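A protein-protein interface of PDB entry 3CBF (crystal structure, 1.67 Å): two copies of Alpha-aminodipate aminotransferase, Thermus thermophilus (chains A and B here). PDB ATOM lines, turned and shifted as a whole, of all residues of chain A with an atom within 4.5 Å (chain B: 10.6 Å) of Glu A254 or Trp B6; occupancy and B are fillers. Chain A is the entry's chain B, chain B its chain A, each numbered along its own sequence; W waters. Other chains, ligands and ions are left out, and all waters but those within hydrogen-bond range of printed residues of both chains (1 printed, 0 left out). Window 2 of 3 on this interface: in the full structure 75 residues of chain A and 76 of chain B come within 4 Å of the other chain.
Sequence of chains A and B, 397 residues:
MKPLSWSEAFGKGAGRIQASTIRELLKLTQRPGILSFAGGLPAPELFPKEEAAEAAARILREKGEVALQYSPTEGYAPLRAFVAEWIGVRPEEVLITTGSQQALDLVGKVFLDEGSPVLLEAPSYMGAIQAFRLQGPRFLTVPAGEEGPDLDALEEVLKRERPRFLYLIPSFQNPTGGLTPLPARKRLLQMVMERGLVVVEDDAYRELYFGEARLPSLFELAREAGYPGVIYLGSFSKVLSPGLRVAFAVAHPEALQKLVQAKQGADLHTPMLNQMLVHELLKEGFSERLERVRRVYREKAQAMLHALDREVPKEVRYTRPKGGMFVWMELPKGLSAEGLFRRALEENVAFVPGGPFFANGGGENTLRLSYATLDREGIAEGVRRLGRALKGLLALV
Water W1 bridges OE2 of Glu A254 (2.6 Å) and N of Ser B7 (2.9 Å).
Hydrophobic or aromatic side chains of chain A within 4 Å of the printed part of chain B: Phe A111, Val A198, His A252 and Ala A255.
Among the printed residues, 13 pairs touch across the chains.
Among the printed residues, no Asp or Glu carboxylate lies within 4 Å of a Lys or Arg side-chain nitrogen of the other chain.
The backbone NH (N) of Glu A254 lies within hydrogen-bond range of a ring nitrogen (ND1) of His A252, at 3.1 Å.
Trp B6 touches Phe A111 (CZ3 to CZ, 3.7 Å).
CD1 of Phe A111 touches O of Ala B9 (3.7 Å).
Phe B10 touches Phe A111 (CD1 to CE1, 3.7 Å).
Phe A111 touches Gly B11.
Trp B6 touches Val A198.
CZ2 of Trp B6 touches O of Pro A228 (3.2 Å).
Glu A254 touches Trp B6 (OE2 to CB, 3.7 Å).
CZ of Phe B10 touches O of Glu A254, 3.7 Å away.
Ala A255 touches Trp B6 (CB to CZ3, 3.8 Å).
CG of Lys A258 touches CZ of Phe B10, 3.8 Å away.
No position is printed for both chains.
Of the 13 pairs that touch across the chains among the printed residues, none has its exchanged pair printed and touching as well.
The indole nitrogen (NE1) of Trp B6 lies within hydrogen-bond range of a ring nitrogen (ND1) of His A252 (3.1 Å).
The backbone carbonyl oxygen of Ala B14 lies within hydrogen-bond range of the side-chain amino group of Lys A258, at 2.8 Å.
O of Ile B17 is in hydrogen-bond range of NZ of Lys A258 (3.1 Å).
Of the printed residues of chain B, Val A198 touches Trp B6 (3.8 Å).
Pro A228 touches just one residue of chain B: Trp B6.
No residue of chain B comes within 4 Å of Pro A253.
Glu A254 touches just these residues of chain B: Trp B6 (3.7 Å) and Phe B10 (3.7 Å).
Ala A255 touches just one residue of chain B: Trp B6 (3.8 Å).
Gln A257 touches none of the printed residues of chain B.
Printed residues of chain B within 4 Å of Lys A258: Phe B10 (3.8 Å), Ala B14 (2.8 Å) and Ile B17 (3.1 Å).
Of chain A, only Phe A111, Val A198, Pro A228, His A252, Glu A254 and Ala A255 come within 4 Å of Trp B6.
Printed residues of chain A within 4 Å of Gly B11: Phe A111.
Printed residues of chain A within 4 Å of Ala B14: Lys A258 (2.8 Å).
Of the printed residues of chain A, Ile B17 touches Lys A258.
The nearest residue of chain B that does not touch Glu A254 is Ser B7 (4.3 Å).
The nearest printed residue of chain A that does not touch Gly B11 is Lys A258 (7.5 Å).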
ATOM      1  N   PHE A 111     -23.521   1.581 -24.634  1.00  0.00           N
ATOM      2  CA  PHE A 111     -23.633   2.983 -25.063  1.00  0.00           C
ATOM      3  C   PHE A 111     -24.559   3.268 -26.235  1.00  0.00           C
ATOM      4  O   PHE A 111     -25.025   4.407 -26.382  1.00  0.00           O
ATOM      5  CB  PHE A 111     -22.245   3.590 -25.304  1.00  0.00           C
ATOM      6  CG  PHE A 111     -21.440   3.738 -24.037  1.00  0.00           C
ATOM      7  CD1 PHE A 111     -21.645   4.824 -23.204  1.00  0.00           C
ATOM      8  CD2 PHE A 111     -20.501   2.771 -23.664  1.00  0.00           C
ATOM      9  CE1 PHE A 111     -20.937   4.945 -22.002  1.00  0.00           C
ATOM     10  CE2 PHE A 111     -19.792   2.891 -22.476  1.00  0.00           C
ATOM     11  CZ  PHE A 111     -19.999   3.981 -21.648  1.00  0.00           C
ATOM     12  N   VAL A 198     -17.501  10.869 -24.081  1.00  0.00           N
ATOM     13  CA  VAL A 198     -16.821   9.606 -23.799  1.00  0.00           C
ATOM     14  C   VAL A 198     -15.898   9.242 -24.953  1.00  0.00           C
ATOM     15  O   VAL A 198     -16.264   9.380 -26.102  1.00  0.00           O
ATOM     16  CB  VAL A 198     -17.855   8.485 -23.602  1.00  0.00           C
ATOM     17  CG1 VAL A 198     -17.170   7.152 -23.318  1.00  0.00           C
ATOM     18  CG2 VAL A 198     -18.763   8.835 -22.424  1.00  0.00           C
ATOM     19  N   PRO A 228     -12.581  11.614 -16.240  1.00  0.00           N
ATOM     20  CA  PRO A 228     -12.928  10.189 -16.154  1.00  0.00           C
ATOM     21  C   PRO A 228     -13.556   9.552 -17.411  1.00  0.00           C
ATOM     22  O   PRO A 228     -13.945   8.367 -17.366  1.00  0.00           O
ATOM     23  CB  PRO A 228     -13.929  10.169 -15.013  1.00  0.00           C
ATOM     24  CG  PRO A 228     -14.728  11.480 -15.257  1.00  0.00           C
ATOM     25  CD  PRO A 228     -13.682  12.476 -15.756  1.00  0.00           C
ATOM     26  N   GLY A 229     -13.632  10.305 -18.512  1.00  0.00           N
ATOM     27  CA  GLY A 229     -14.380   9.832 -19.669  1.00  0.00           C
ATOM     28  C   GLY A 229     -13.690   8.947 -20.708  1.00  0.00           C
ATOM     29  O   GLY A 229     -14.301   8.660 -21.729  1.00  0.00           O
ATOM     30  N   HIS A 252     -13.643   4.094 -15.589  1.00  0.00           N
ATOM     31  CA  HIS A 252     -14.233   4.597 -14.355  1.00  0.00           C
ATOM     32  C   HIS A 252     -15.174   3.516 -13.795  1.00  0.00           C
ATOM     33  O   HIS A 252     -15.812   2.825 -14.559  1.00  0.00           O
ATOM     34  CB  HIS A 252     -15.016   5.858 -14.728  1.00  0.00           C
ATOM     35  CG  HIS A 252     -15.738   6.493 -13.591  1.00  0.00           C
ATOM     36  ND1 HIS A 252     -16.991   6.088 -13.171  1.00  0.00           N
ATOM     37  CD2 HIS A 252     -15.403   7.551 -12.820  1.00  0.00           C
ATOM     38  CE1 HIS A 252     -17.379   6.849 -12.165  1.00  0.00           C
ATOM     39  NE2 HIS A 252     -16.440   7.758 -11.945  1.00  0.00           N
ATOM     40  N   PRO A 253     -15.250   3.345 -12.453  1.00  0.00           N
ATOM     41  CA  PRO A 253     -16.087   2.312 -11.840  1.00  0.00           C
ATOM     42  C   PRO A 253     -17.503   2.149 -12.366  1.00  0.00           C
ATOM     43  O   PRO A 253     -17.997   1.013 -12.411  1.00  0.00           O
ATOM     44  CB  PRO A 253     -16.179   2.785 -10.378  1.00  0.00           C
ATOM     45  CG  PRO A 253     -14.897   3.421 -10.157  1.00  0.00           C
ATOM     46  CD  PRO A 253     -14.546   4.131 -11.419  1.00  0.00           C
ATOM     47  N   GLU A 254     -18.184   3.252 -12.695  1.00  0.00           N
ATOM     48  CA  GLU A 254     -19.567   3.129 -13.163  1.00  0.00           C
ATOM     49  C   GLU A 254     -19.590   2.476 -14.531  1.00  0.00           C
ATOM     50  O   GLU A 254     -20.412   1.581 -14.804  1.00  0.00           O
ATOM     51  CB  GLU A 254     -20.283   4.471 -13.229  1.00  0.00           C
ATOM     52  CG  GLU A 254     -20.860   4.937 -11.888  1.00  0.00           C
ATOM     53  CD  GLU A 254     -21.654   6.217 -12.033  1.00  0.00           C
ATOM     54  OE1 GLU A 254     -21.100   7.297 -11.714  1.00  0.00           O
ATOM     55  OE2 GLU A 254     -22.808   6.135 -12.508  1.00  0.00           O
ATOM     56  N   ALA A 255     -18.692   2.930 -15.398  1.00  0.00           N
ATOM     57  CA  ALA A 255     -18.651   2.365 -16.760  1.00  0.00           C
ATOM     58  C   ALA A 255     -18.120   0.937 -16.648  1.00  0.00           C
ATOM     59  O   ALA A 255     -18.670   0.017 -17.269  1.00  0.00           O
ATOM     60  CB  ALA A 255     -17.807   3.188 -17.677  1.00  0.00           C
ATOM     61  N   LEU A 256     -17.104   0.731 -15.813  1.00  0.00           N
ATOM     62  CA  LEU A 256     -16.556  -0.607 -15.638  1.00  0.00           C
ATOM     63  C   LEU A 256     -17.591  -1.618 -15.128  1.00  0.00           C
ATOM     64  O   LEU A 256     -17.602  -2.781 -15.580  1.00  0.00           O
ATOM     65  CB  LEU A 256     -15.324  -0.583 -14.727  1.00  0.00           C
ATOM     66  CG  LEU A 256     -14.486  -1.875 -14.752  1.00  0.00           C
ATOM     67  CD1 LEU A 256     -13.775  -2.001 -16.109  1.00  0.00           C
ATOM     68  CD2 LEU A 256     -13.486  -1.946 -13.606  1.00  0.00           C
ATOM     69  N   GLN A 257     -18.467  -1.189 -14.215  1.00  0.00           N
ATOM     70  CA  GLN A 257     -19.478  -2.098 -13.660  1.00  0.00           C
ATOM     71  C   GLN A 257     -20.426  -2.580 -14.751  1.00  0.00           C
ATOM     72  O   GLN A 257     -20.772  -3.759 -14.801  1.00  0.00           O
ATOM     73  CB  GLN A 257     -20.282  -1.439 -12.530  1.00  0.00           C
ATOM     74  CG  GLN A 257     -21.317  -2.379 -11.942  1.00  0.00           C
ATOM     75  CD  GLN A 257     -22.161  -1.731 -10.874  1.00  0.00           C
ATOM     76  OE1 GLN A 257     -22.987  -0.857 -11.160  1.00  0.00           O
ATOM     77  NE2 GLN A 257     -21.953  -2.146  -9.636  1.00  0.00           N
ATOM     78  N   LYS A 258     -20.880  -1.657 -15.595  1.00  0.00           N
ATOM     79  CA  LYS A 258     -21.738  -2.029 -16.707  1.00  0.00           C
ATOM     80  C   LYS A 258     -21.033  -2.974 -17.690  1.00  0.00           C
ATOM     81  O   LYS A 258     -21.645  -3.921 -18.188  1.00  0.00           O
ATOM     82  CB  LYS A 258     -22.287  -0.813 -17.445  1.00  0.00           C
ATOM     83  CG  LYS A 258     -23.298  -0.046 -16.635  1.00  0.00           C
ATOM     84  CD  LYS A 258     -24.537  -0.868 -16.317  1.00  0.00           C
ATOM     85  CE  LYS A 258     -25.488  -0.017 -15.489  1.00  0.00           C
ATOM     86  NZ  LYS A 258     -26.720  -0.769 -15.156  1.00  0.00           N
ATOM     87  N   SER B   5     -24.235  11.615 -14.819  1.00  0.00           N
ATOM     88  CA  SER B   5     -22.983  11.751 -15.636  1.00  0.00           C
ATOM     89  C   SER B   5     -22.896  10.499 -16.503  1.00  0.00           C
ATOM     90  O   SER B   5     -23.314  10.543 -17.654  1.00  0.00           O
ATOM     91  CB  SER B   5     -21.733  11.925 -14.754  1.00  0.00           C
ATOM     92  OG  SER B   5     -20.728  12.723 -15.402  1.00  0.00           O
ATOM     93  N   TRP B   6     -22.394   9.387 -15.949  1.00  0.00           N
ATOM     94  CA  TRP B   6     -22.461   8.072 -16.648  1.00  0.00           C
ATOM     95  C   TRP B   6     -23.885   7.601 -16.945  1.00  0.00           C
ATOM     96  O   TRP B   6     -24.168   7.142 -18.048  1.00  0.00           O
ATOM     97  CB  TRP B   6     -21.673   6.980 -15.921  1.00  0.00           C
ATOM     98  CG  TRP B   6     -20.219   7.227 -16.008  1.00  0.00           C
ATOM     99  CD1 TRP B   6     -19.419   7.715 -15.021  1.00  0.00           C
ATOM    100  CD2 TRP B   6     -19.381   7.047 -17.162  1.00  0.00           C
ATOM    101  NE1 TRP B   6     -18.130   7.836 -15.479  1.00  0.00           N
ATOM    102  CE2 TRP B   6     -18.079   7.440 -16.793  1.00  0.00           C
ATOM    103  CE3 TRP B   6     -19.610   6.609 -18.474  1.00  0.00           C
ATOM    104  CZ2 TRP B   6     -16.994   7.386 -17.685  1.00  0.00           C
ATOM    105  CZ3 TRP B   6     -18.539   6.555 -19.364  1.00  0.00           C
ATOM    106  CH2 TRP B   6     -17.238   6.938 -18.964  1.00  0.00           C
ATOM    107  N   SER B   7     -24.792   7.745 -15.978  1.00  0.00           N
ATOM    108  CA  SER B   7     -26.188   7.367 -16.218  1.00  0.00           C
ATOM    109  C   SER B   7     -26.810   8.124 -17.413  1.00  0.00           C
ATOM    110  O   SER B   7     -27.575   7.542 -18.186  1.00  0.00           O
ATOM    111  CB  SER B   7     -27.027   7.490 -14.935  1.00  0.00           C
ATOM    112  OG  SER B   7     -26.990   8.808 -14.419  1.00  0.00           O
ATOM    113  N   GLU B   8     -26.446   9.394 -17.574  1.00  0.00           N
ATOM    114  CA  GLU B   8     -26.882  10.208 -18.711  1.00  0.00           C
ATOM    115  C   GLU B   8     -26.191   9.776 -20.010  1.00  0.00           C
ATOM    116  O   GLU B   8     -26.795   9.791 -21.083  1.00  0.00           O
ATOM    117  CB  GLU B   8     -26.612  11.693 -18.427  1.00  0.00           C
ATOM    118  CG  GLU B   8     -27.314  12.666 -19.367  1.00  0.00           C
ATOM    119  CD  GLU B   8     -28.680  13.102 -18.851  1.00  0.00           C
ATOM    120  OE1 GLU B   8     -28.757  14.210 -18.261  1.00  0.00           O
ATOM    121  OE2 GLU B   8     -29.667  12.345 -19.032  1.00  0.00           O
ATOM    122  N   ALA B   9     -24.921   9.381 -19.894  1.00  0.00           N
ATOM    123  CA  ALA B   9     -24.107   8.949 -21.026  1.00  0.00           C
ATOM    124  C   ALA B   9     -24.489   7.558 -21.569  1.00  0.00           C
ATOM    125  O   ALA B   9     -24.372   7.303 -22.766  1.00  0.00           O
ATOM    126  CB  ALA B   9     -22.605   8.972 -20.622  1.00  0.00           C
ATOM    127  N   PHE B  10     -24.911   6.660 -20.679  1.00  0.00           N
ATOM    128  CA  PHE B  10     -25.291   5.298 -21.054  1.00  0.00           C
ATOM    129  C   PHE B  10     -26.421   5.237 -22.050  1.00  0.00           C
ATOM    130  O   PHE B  10     -27.286   6.127 -22.071  1.00  0.00           O
ATOM    131  CB  PHE B  10     -25.710   4.493 -19.824  1.00  0.00           C
ATOM    132  CG  PHE B  10     -24.587   4.188 -18.885  1.00  0.00           C
ATOM    133  CD1 PHE B  10     -23.296   4.009 -19.361  1.00  0.00           C
ATOM    134  CD2 PHE B  10     -24.826   4.058 -17.516  1.00  0.00           C
ATOM    135  CE1 PHE B  10     -22.267   3.727 -18.492  1.00  0.00           C
ATOM    136  CE2 PHE B  10     -23.807   3.781 -16.632  1.00  0.00           C
ATOM    137  CZ  PHE B  10     -22.514   3.612 -17.117  1.00  0.00           C
ATOM    138  N   GLY B  11     -26.425   4.175 -22.855  1.00  0.00           N
ATOM    139  CA  GLY B  11     -27.543   3.901 -23.746  1.00  0.00           C
ATOM    140  C   GLY B  11     -28.620   3.110 -23.023  1.00  0.00           C
ATOM    141  O   GLY B  11     -28.474   2.759 -21.842  1.00  0.00           O
ATOM    142  N   LYS B  12     -29.709   2.823 -23.738  1.00  0.00           N
ATOM    143  CA  LYS B  12     -30.832   2.100 -23.152  1.00  0.00           C
ATOM    144  C   LYS B  12     -30.433   0.714 -22.665  1.00  0.00           C
ATOM    145  O   LYS B  12     -31.044   0.181 -21.736  1.00  0.00           O
ATOM    146  CB  LYS B  12     -31.994   1.985 -24.146  1.00  0.00           C
ATOM    147  CG  LYS B  12     -32.676   3.306 -24.487  1.00  0.00           C
ATOM    148  CD  LYS B  12     -33.861   3.081 -25.421  1.00  0.00           C
ATOM    149  CE  LYS B  12     -34.736   4.353 -25.473  1.00  0.00           C
ATOM    150  NZ  LYS B  12     -35.861   4.232 -26.469  1.00  0.00           N
ATOM    151  N   GLY B  13     -29.405   0.139 -23.295  1.00  0.00           N
ATOM    152  CA  GLY B  13     -28.865  -1.170 -22.906  1.00  0.00           C
ATOM    153  C   GLY B  13     -28.323  -1.222 -21.492  1.00  0.00           C
ATOM    154  O   GLY B  13     -28.546  -2.186 -20.766  1.00  0.00           O
ATOM    155  N   ALA B  14     -27.609  -0.180 -21.084  1.00  0.00           N
ATOM    156  CA  ALA B  14     -27.113  -0.100 -19.718  1.00  0.00           C
ATOM    157  C   ALA B  14     -28.225  -0.220 -18.655  1.00  0.00           C
ATOM    158  O   ALA B  14     -28.015  -0.804 -17.597  1.00  0.00           O
ATOM    159  CB  ALA B  14     -26.321   1.180 -19.525  1.00  0.00           C
ATOM    160  N   GLY B  15     -29.414   0.316 -18.951  1.00  0.00           N
ATOM    161  CA  GLY B  15     -30.544   0.185 -18.034  1.00  0.00           C
ATOM    162  C   GLY B  15     -31.152  -1.208 -17.957  1.00  0.00           C
ATOM    163  O   GLY B  15     -31.828  -1.546 -16.990  1.00  0.00           O
ATOM    164  N   ILE B  17     -29.148  -3.844 -18.284  1.00  0.00           N
ATOM    165  CA  ILE B  17     -28.020  -4.624 -17.753  1.00  0.00           C
ATOM    166  C   ILE B  17     -28.100  -4.609 -16.213  1.00  0.00           C
ATOM    167  O   ILE B  17     -28.153  -3.532 -15.603  1.00  0.00           O
ATOM    168  CB  ILE B  17     -26.684  -4.039 -18.249  1.00  0.00           C
ATOM    169  CG1 ILE B  17     -26.472  -4.356 -19.738  1.00  0.00           C
ATOM    170  CG2 ILE B  17     -25.519  -4.605 -17.468  1.00  0.00           C
ATOM    171  CD1 ILE B  17     -25.336  -3.539 -20.419  1.00  0.00           C
HETATM  172  O   HOH W   1     -24.394   8.074 -13.109  1.00  0.00           O
